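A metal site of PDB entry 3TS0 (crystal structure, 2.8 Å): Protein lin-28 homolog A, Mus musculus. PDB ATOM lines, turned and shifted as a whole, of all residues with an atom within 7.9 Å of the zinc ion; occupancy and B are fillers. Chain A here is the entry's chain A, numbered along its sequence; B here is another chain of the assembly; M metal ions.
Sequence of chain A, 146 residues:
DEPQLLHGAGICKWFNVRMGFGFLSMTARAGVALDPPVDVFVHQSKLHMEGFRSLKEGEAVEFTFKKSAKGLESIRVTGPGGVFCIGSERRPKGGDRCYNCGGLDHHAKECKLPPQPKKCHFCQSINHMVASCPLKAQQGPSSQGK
Within 4 Å of the zinc ion: Cys 120, Cys 123, His 128 and Cys 133.
The nearest printed residue that does not touch the zinc ion is Ser 125 (4.6 Å).
The zinc ion is bound by NE2 of His 128 (1.9 Å).
SG of Cys 123 is bound to the zinc ion (2.2 Å).
The side-chain sulfur (SG) of Cys 133 binds the zinc ion.
The zinc ion is bound by the side-chain sulfur (SG) of Cys 120.
ND1 of His 128 lies within hydrogen-bond range of OG of Ser 125, at 3.3 Å.
The side-chain sulfur (SG) of Cys 123 lies close to the backbone NH (N) of Ser 125.
N of Ala 60 sits at hydrogen-bond distance from O of Cys 123 (3.0 Å).
The backbone NH of Leu 135 lies close to the side-chain sulfur of Cys 133 (3.6 Å).
SG of Cys 133 lies close to N of Lys 136 (3.4 Å).
The backbone carbonyl oxygen (O) of Ser 125 sits at hydrogen-bond distance from the backbone NH (N) of Cys 120 (2.7 Å).
The backbone NH of Phe 122 sits close to the side-chain sulfur of Cys 120, at 3.4 Å.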
ATOM      1  N   GLY A  58      28.453   2.057  12.124  1.00  0.00           N
ATOM      2  CA  GLY A  58      29.078   1.747  10.838  1.00  0.00           C
ATOM      3  C   GLY A  58      28.740   2.643   9.660  1.00  0.00           C
ATOM      4  O   GLY A  58      29.429   2.605   8.633  1.00  0.00           O
ATOM      5  N   GLU A  59      27.698   3.480   9.784  1.00  0.00           N
ATOM      6  CA  GLU A  59      27.348   4.358   8.682  1.00  0.00           C
ATOM      7  C   GLU A  59      28.442   5.424   8.453  1.00  0.00           C
ATOM      8  O   GLU A  59      29.030   5.906   9.422  1.00  0.00           O
ATOM      9  CB  GLU A  59      25.937   4.936   8.835  1.00  0.00           C
ATOM     10  CG  GLU A  59      25.718   6.030   9.879  1.00  0.00           C
ATOM     11  CD  GLU A  59      24.537   6.907   9.485  1.00  0.00           C
ATOM     12  OE1 GLU A  59      23.443   6.714  10.053  1.00  0.00           O
ATOM     13  OE2 GLU A  59      24.692   7.717   8.534  1.00  0.00           O
ATOM     14  N   ALA A  60      28.793   5.653   7.175  1.00  0.00           N
ATOM     15  CA  ALA A  60      29.774   6.580   6.643  1.00  0.00           C
ATOM     16  C   ALA A  60      29.349   8.039   6.868  1.00  0.00           C
ATOM     17  O   ALA A  60      28.245   8.428   6.508  1.00  0.00           O
ATOM     18  CB  ALA A  60      29.937   6.322   5.166  1.00  0.00           C
ATOM     19  N   ILE A  86      21.785   8.102   7.716  1.00  0.00           N
ATOM     20  CA  ILE A  86      20.842   6.994   7.669  1.00  0.00           C
ATOM     21  C   ILE A  86      20.012   6.894   8.959  1.00  0.00           C
ATOM     22  O   ILE A  86      18.785   6.834   8.892  1.00  0.00           O
ATOM     23  CB  ILE A  86      21.591   5.685   7.344  1.00  0.00           C
ATOM     24  CG1 ILE A  86      22.091   5.677   5.897  1.00  0.00           C
ATOM     25  CG2 ILE A  86      20.744   4.450   7.656  1.00  0.00           C
ATOM     26  CD1 ILE A  86      23.239   4.782   5.683  1.00  0.00           C
ATOM     27  N   LYS A 119      26.784   5.904  -3.498  1.00  0.00           N
ATOM     28  CA  LYS A 119      27.043   5.507  -2.115  1.00  0.00           C
ATOM     29  C   LYS A 119      26.260   4.244  -1.679  1.00  0.00           C
ATOM     30  O   LYS A 119      25.171   4.025  -2.181  1.00  0.00           O
ATOM     31  CB  LYS A 119      27.036   6.724  -1.158  1.00  0.00           C
ATOM     32  CG  LYS A 119      25.703   7.312  -0.794  1.00  0.00           C
ATOM     33  CD  LYS A 119      25.849   8.771  -0.355  1.00  0.00           C
ATOM     34  CE  LYS A 119      25.648   9.763  -1.485  1.00  0.00           C
ATOM     35  NZ  LYS A 119      24.269   9.684  -2.042  1.00  0.00           N
ATOM     36  N   CYS A 120      26.876   3.339  -0.866  1.00  0.00           N
ATOM     37  CA  CYS A 120      26.282   2.046  -0.453  1.00  0.00           C
ATOM     38  C   CYS A 120      24.846   2.184  -0.037  1.00  0.00           C
ATOM     39  O   CYS A 120      24.493   3.104   0.686  1.00  0.00           O
ATOM     40  CB  CYS A 120      27.107   1.392   0.644  1.00  0.00           C
ATOM     41  SG  CYS A 120      26.519  -0.237   1.172  1.00  0.00           S
ATOM     42  N   HIS A 121      24.014   1.254  -0.487  1.00  0.00           N
ATOM     43  CA  HIS A 121      22.586   1.236  -0.143  1.00  0.00           C
ATOM     44  C   HIS A 121      22.335   0.927   1.334  1.00  0.00           C
ATOM     45  O   HIS A 121      21.260   1.238   1.845  1.00  0.00           O
ATOM     46  CB  HIS A 121      21.859   0.235  -1.016  1.00  0.00           C
ATOM     47  CG  HIS A 121      21.595   0.673  -2.416  1.00  0.00           C
ATOM     48  ND1 HIS A 121      21.522  -0.240  -3.452  1.00  0.00           N
ATOM     49  CD2 HIS A 121      21.330   1.905  -2.902  1.00  0.00           C
ATOM     50  CE1 HIS A 121      21.249   0.459  -4.537  1.00  0.00           C
ATOM     51  NE2 HIS A 121      21.120   1.756  -4.262  1.00  0.00           N
ATOM     52  N   PHE A 122      23.321   0.310   2.038  1.00  0.00           N
ATOM     53  CA  PHE A 122      23.189  -0.039   3.441  1.00  0.00           C
ATOM     54  C   PHE A 122      23.895   0.921   4.398  1.00  0.00           C
ATOM     55  O   PHE A 122      23.330   1.265   5.420  1.00  0.00           O
ATOM     56  CB  PHE A 122      23.658  -1.482   3.675  1.00  0.00           C
ATOM     57  CG  PHE A 122      23.397  -2.026   5.049  1.00  0.00           C
ATOM     58  CD1 PHE A 122      22.114  -2.454   5.417  1.00  0.00           C
ATOM     59  CD2 PHE A 122      24.426  -2.190   5.972  1.00  0.00           C
ATOM     60  CE1 PHE A 122      21.859  -2.975   6.690  1.00  0.00           C
ATOM     61  CE2 PHE A 122      24.181  -2.710   7.247  1.00  0.00           C
ATOM     62  CZ  PHE A 122      22.893  -3.097   7.598  1.00  0.00           C
ATOM     63  N   CYS A 123      25.127   1.329   4.092  1.00  0.00           N
ATOM     64  CA  CYS A 123      25.930   2.131   5.003  1.00  0.00           C
ATOM     65  C   CYS A 123      26.379   3.470   4.440  1.00  0.00           C
ATOM     66  O   CYS A 123      27.170   4.141   5.099  1.00  0.00           O
ATOM     67  CB  CYS A 123      27.135   1.308   5.473  1.00  0.00           C
ATOM     68  SG  CYS A 123      28.408   1.084   4.198  1.00  0.00           S
ATOM     69  N   GLN A 124      25.993   3.817   3.212  1.00  0.00           N
ATOM     70  CA  GLN A 124      26.395   5.081   2.554  1.00  0.00           C
ATOM     71  C   GLN A 124      27.860   5.246   2.235  1.00  0.00           C
ATOM     72  O   GLN A 124      28.261   6.326   1.816  1.00  0.00           O
ATOM     73  CB  GLN A 124      25.881   6.309   3.281  1.00  0.00           C
ATOM     74  CG  GLN A 124      24.475   6.676   2.841  1.00  0.00           C
ATOM     75  CD  GLN A 124      23.977   7.925   3.520  1.00  0.00           C
ATOM     76  OE1 GLN A 124      23.079   8.561   3.023  1.00  0.00           O
ATOM     77  NE2 GLN A 124      24.556   8.291   4.694  1.00  0.00           N
ATOM     78  N   SER A 125      28.673   4.189   2.380  1.00  0.00           N
ATOM     79  CA  SER A 125      30.072   4.291   1.991  1.00  0.00           C
ATOM     80  C   SER A 125      30.163   4.582   0.494  1.00  0.00           C
ATOM     81  O   SER A 125      29.364   4.073  -0.289  1.00  0.00           O
ATOM     82  CB  SER A 125      30.819   3.009   2.281  1.00  0.00           C
ATOM     83  OG  SER A 125      32.097   3.026   1.666  1.00  0.00           O
ATOM     84  N   ILE A 126      31.132   5.396   0.130  1.00  0.00           N
ATOM     85  CA  ILE A 126      31.431   5.742  -1.272  1.00  0.00           C
ATOM     86  C   ILE A 126      32.542   4.837  -1.792  1.00  0.00           C
ATOM     87  O   ILE A 126      32.977   5.015  -2.926  1.00  0.00           O
ATOM     88  CB  ILE A 126      31.812   7.231  -1.421  1.00  0.00           C
ATOM     89  CG1 ILE A 126      33.084   7.564  -0.571  1.00  0.00           C
ATOM     90  CG2 ILE A 126      30.624   8.142  -1.086  1.00  0.00           C
ATOM     91  CD1 ILE A 126      33.868   8.773  -1.055  1.00  0.00           C
ATOM     92  N   ASN A 127      33.024   3.893  -0.949  1.00  0.00           N
ATOM     93  CA  ASN A 127      34.150   3.000  -1.255  1.00  0.00           C
ATOM     94  C   ASN A 127      33.725   1.633  -1.751  1.00  0.00           C
ATOM     95  O   ASN A 127      34.524   0.925  -2.383  1.00  0.00           O
ATOM     96  CB  ASN A 127      35.097   2.899  -0.063  1.00  0.00           C
ATOM     97  CG  ASN A 127      35.726   4.224   0.306  1.00  0.00           C
ATOM     98  OD1 ASN A 127      36.247   4.976  -0.540  1.00  0.00           O
ATOM     99  ND2 ASN A 127      35.686   4.527   1.598  1.00  0.00           N
ATOM    100  N   HIS A 128      32.449   1.265  -1.478  1.00  0.00           N
ATOM    101  CA  HIS A 128      31.889   0.007  -1.892  1.00  0.00           C
ATOM    102  C   HIS A 128      30.400   0.106  -2.211  1.00  0.00           C
ATOM    103  O   HIS A 128      29.753   1.132  -1.977  1.00  0.00           O
ATOM    104  CB  HIS A 128      32.156  -1.071  -0.838  1.00  0.00           C
ATOM    105  CG  HIS A 128      31.385  -0.886   0.426  1.00  0.00           C
ATOM    106  ND1 HIS A 128      31.964  -0.308   1.535  1.00  0.00           N
ATOM    107  CD2 HIS A 128      30.094  -1.172   0.693  1.00  0.00           C
ATOM    108  CE1 HIS A 128      31.018  -0.285   2.462  1.00  0.00           C
ATOM    109  NE2 HIS A 128      29.864  -0.774   1.998  1.00  0.00           N
ATOM    110  N   MET A 129      29.865  -1.017  -2.733  1.00  0.00           N
ATOM    111  CA  MET A 129      28.467  -1.152  -3.046  1.00  0.00           C
ATOM    112  C   MET A 129      27.852  -2.279  -2.215  1.00  0.00           C
ATOM    113  O   MET A 129      28.600  -3.059  -1.609  1.00  0.00           O
ATOM    114  CB  MET A 129      28.260  -1.295  -4.522  1.00  0.00           C
ATOM    115  CG  MET A 129      28.404   0.005  -5.180  1.00  0.00           C
ATOM    116  SD  MET A 129      28.177  -0.106  -6.937  1.00  0.00           S
ATOM    117  CE  MET A 129      28.324   1.668  -7.357  1.00  0.00           C
ATOM    118  N   VAL A 130      26.530  -2.285  -2.088  1.00  0.00           N
ATOM    119  CA  VAL A 130      25.834  -3.175  -1.168  1.00  0.00           C
ATOM    120  C   VAL A 130      26.190  -4.644  -1.255  1.00  0.00           C
ATOM    121  O   VAL A 130      26.421  -5.247  -0.219  1.00  0.00           O
ATOM    122  CB  VAL A 130      24.333  -2.860  -1.012  1.00  0.00           C
ATOM    123  CG1 VAL A 130      23.547  -3.259  -2.260  1.00  0.00           C
ATOM    124  CG2 VAL A 130      23.770  -3.494   0.248  1.00  0.00           C
ATOM    125  N   ALA A 131      26.396  -5.199  -2.488  1.00  0.00           N
ATOM    126  CA  ALA A 131      26.778  -6.612  -2.658  1.00  0.00           C
ATOM    127  C   ALA A 131      28.148  -6.925  -2.104  1.00  0.00           C
ATOM    128  O   ALA A 131      28.540  -8.093  -2.027  1.00  0.00           O
ATOM    129  CB  ALA A 131      26.694  -7.003  -4.113  1.00  0.00           C
ATOM    130  N   SER A 132      28.894  -5.906  -1.684  1.00  0.00           N
ATOM    131  CA  SER A 132      30.228  -6.073  -1.107  1.00  0.00           C
ATOM    132  C   SER A 132      30.361  -5.315   0.194  1.00  0.00           C
ATOM    133  O   SER A 132      31.463  -4.957   0.592  1.00  0.00           O
ATOM    134  CB  SER A 132      31.283  -5.610  -2.106  1.00  0.00           C
ATOM    135  OG  SER A 132      31.322  -6.471  -3.227  1.00  0.00           O
ATOM    136  N   CYS A 133      29.215  -5.071   0.858  1.00  0.00           N
ATOM    137  CA  CYS A 133      29.179  -4.344   2.101  1.00  0.00           C
ATOM    138  C   CYS A 133      29.678  -5.111   3.318  1.00  0.00           C
ATOM    139  O   CYS A 133      28.976  -6.021   3.803  1.00  0.00           O
ATOM    140  CB  CYS A 133      27.820  -3.705   2.335  1.00  0.00           C
ATOM    141  SG  CYS A 133      27.751  -2.683   3.828  1.00  0.00           S
ATOM    142  N   PRO A 134      30.843  -4.713   3.874  1.00  0.00           N
ATOM    143  CA  PRO A 134      31.330  -5.374   5.092  1.00  0.00           C
ATOM    144  C   PRO A 134      30.415  -5.236   6.298  1.00  0.00           C
ATOM    145  O   PRO A 134      30.295  -6.175   7.065  1.00  0.00           O
ATOM    146  CB  PRO A 134      32.711  -4.748   5.334  1.00  0.00           C
ATOM    147  CG  PRO A 134      32.759  -3.537   4.527  1.00  0.00           C
ATOM    148  CD  PRO A 134      31.755  -3.649   3.424  1.00  0.00           C
ATOM    149  N   LEU A 135      29.711  -4.092   6.435  1.00  0.00           N
ATOM    150  CA  LEU A 135      28.772  -3.881   7.531  1.00  0.00           C
ATOM    151  C   LEU A 135      27.540  -4.806   7.428  1.00  0.00           C
ATOM    152  O   LEU A 135      27.219  -5.457   8.408  1.00  0.00           O
ATOM    153  CB  LEU A 135      28.353  -2.410   7.619  1.00  0.00           C
ATOM    154  CG  LEU A 135      27.508  -2.046   8.854  1.00  0.00           C
ATOM    155  CD1 LEU A 135      28.352  -2.117  10.152  1.00  0.00           C
ATOM    156  CD2 LEU A 135      26.809  -0.679   8.695  1.00  0.00           C
ATOM    157  N   LYS A 136      26.901  -4.881   6.245  1.00  0.00           N
ATOM    158  CA  LYS A 136      25.721  -5.740   6.027  1.00  0.00           C
ATOM    159  C   LYS A 136      26.073  -7.200   6.243  1.00  0.00           C
ATOM    160  O   LYS A 136      25.220  -7.963   6.696  1.00  0.00           O
ATOM    161  CB  LYS A 136      25.108  -5.537   4.638  1.00  0.00           C
ATOM    162  CG  LYS A 136      23.728  -6.125   4.497  1.00  0.00           C
ATOM    163  CD  LYS A 136      23.283  -6.211   3.053  1.00  0.00           C
ATOM    164  CE  LYS A 136      21.823  -6.546   2.937  1.00  0.00           C
ATOM    165  NZ  LYS A 136      21.383  -6.586   1.521  1.00  0.00           N
ATOM    166  N   ALA A 137      27.350  -7.575   5.974  1.00  0.00           N
ATOM    167  CA  ALA A 137      27.876  -8.922   6.189  1.00  0.00           C
ATOM    168  C   ALA A 137      28.083  -9.203   7.701  1.00  0.00           C
ATOM    169  O   ALA A 137      29.182  -9.544   8.131  1.00  0.00           O
ATOM    170  CB  ALA A 137      29.196  -9.059   5.435  1.00  0.00           C
ATOM    171  P     G B  20      23.236  -3.974 -10.377  1.00  0.00           P
ATOM    172  OP1   G B  20      22.973  -4.875 -11.513  1.00  0.00           O
ATOM    173  OP2   G B  20      24.457  -4.159  -9.549  1.00  0.00           O
ATOM    174  O5'   G B  20      23.313  -2.494 -10.955  1.00  0.00           O
ATOM    175  C5'   G B  20      22.176  -1.627 -10.955  1.00  0.00           C
ATOM    176  C4'   G B  20      22.623  -0.217 -10.608  1.00  0.00           C
ATOM    177  O4'   G B  20      22.654  -0.040  -9.172  1.00  0.00           O
ATOM    178  C3'   G B  20      24.019   0.121 -11.121  1.00  0.00           C
ATOM    179  O3'   G B  20      23.993   1.424 -11.672  1.00  0.00           O
ATOM    180  C2'   G B  20      24.887  -0.007  -9.873  1.00  0.00           C
ATOM    181  O2'   G B  20      26.129   0.657  -9.896  1.00  0.00           O
ATOM    182  C1'   G B  20      23.913   0.512  -8.825  1.00  0.00           C
ATOM    183  N9    G B  20      24.225   0.088  -7.465  1.00  0.00           N
ATOM    184  C8    G B  20      24.416  -1.205  -7.008  1.00  0.00           C
ATOM    185  N7    G B  20      24.637  -1.277  -5.725  1.00  0.00           N
ATOM    186  C5    G B  20      24.598   0.042  -5.308  1.00  0.00           C
ATOM    187  C6    G B  20      24.753   0.595  -4.003  1.00  0.00           C
ATOM    188  O6    G B  20      24.997  -0.019  -2.964  1.00  0.00           O
ATOM    189  N1    G B  20      24.530   1.985  -3.970  1.00  0.00           N
ATOM    190  C2    G B  20      24.218   2.747  -5.081  1.00  0.00           C
ATOM    191  N2    G B  20      24.112   4.085  -4.904  1.00  0.00           N
ATOM    192  N3    G B  20      24.128   2.249  -6.308  1.00  0.00           N
ATOM    193  C4    G B  20      24.336   0.898  -6.360  1.00  0.00           C
HETATM  194 ZN    ZN M   1      28.127  -0.650   2.811  1.00  0.00          ZN
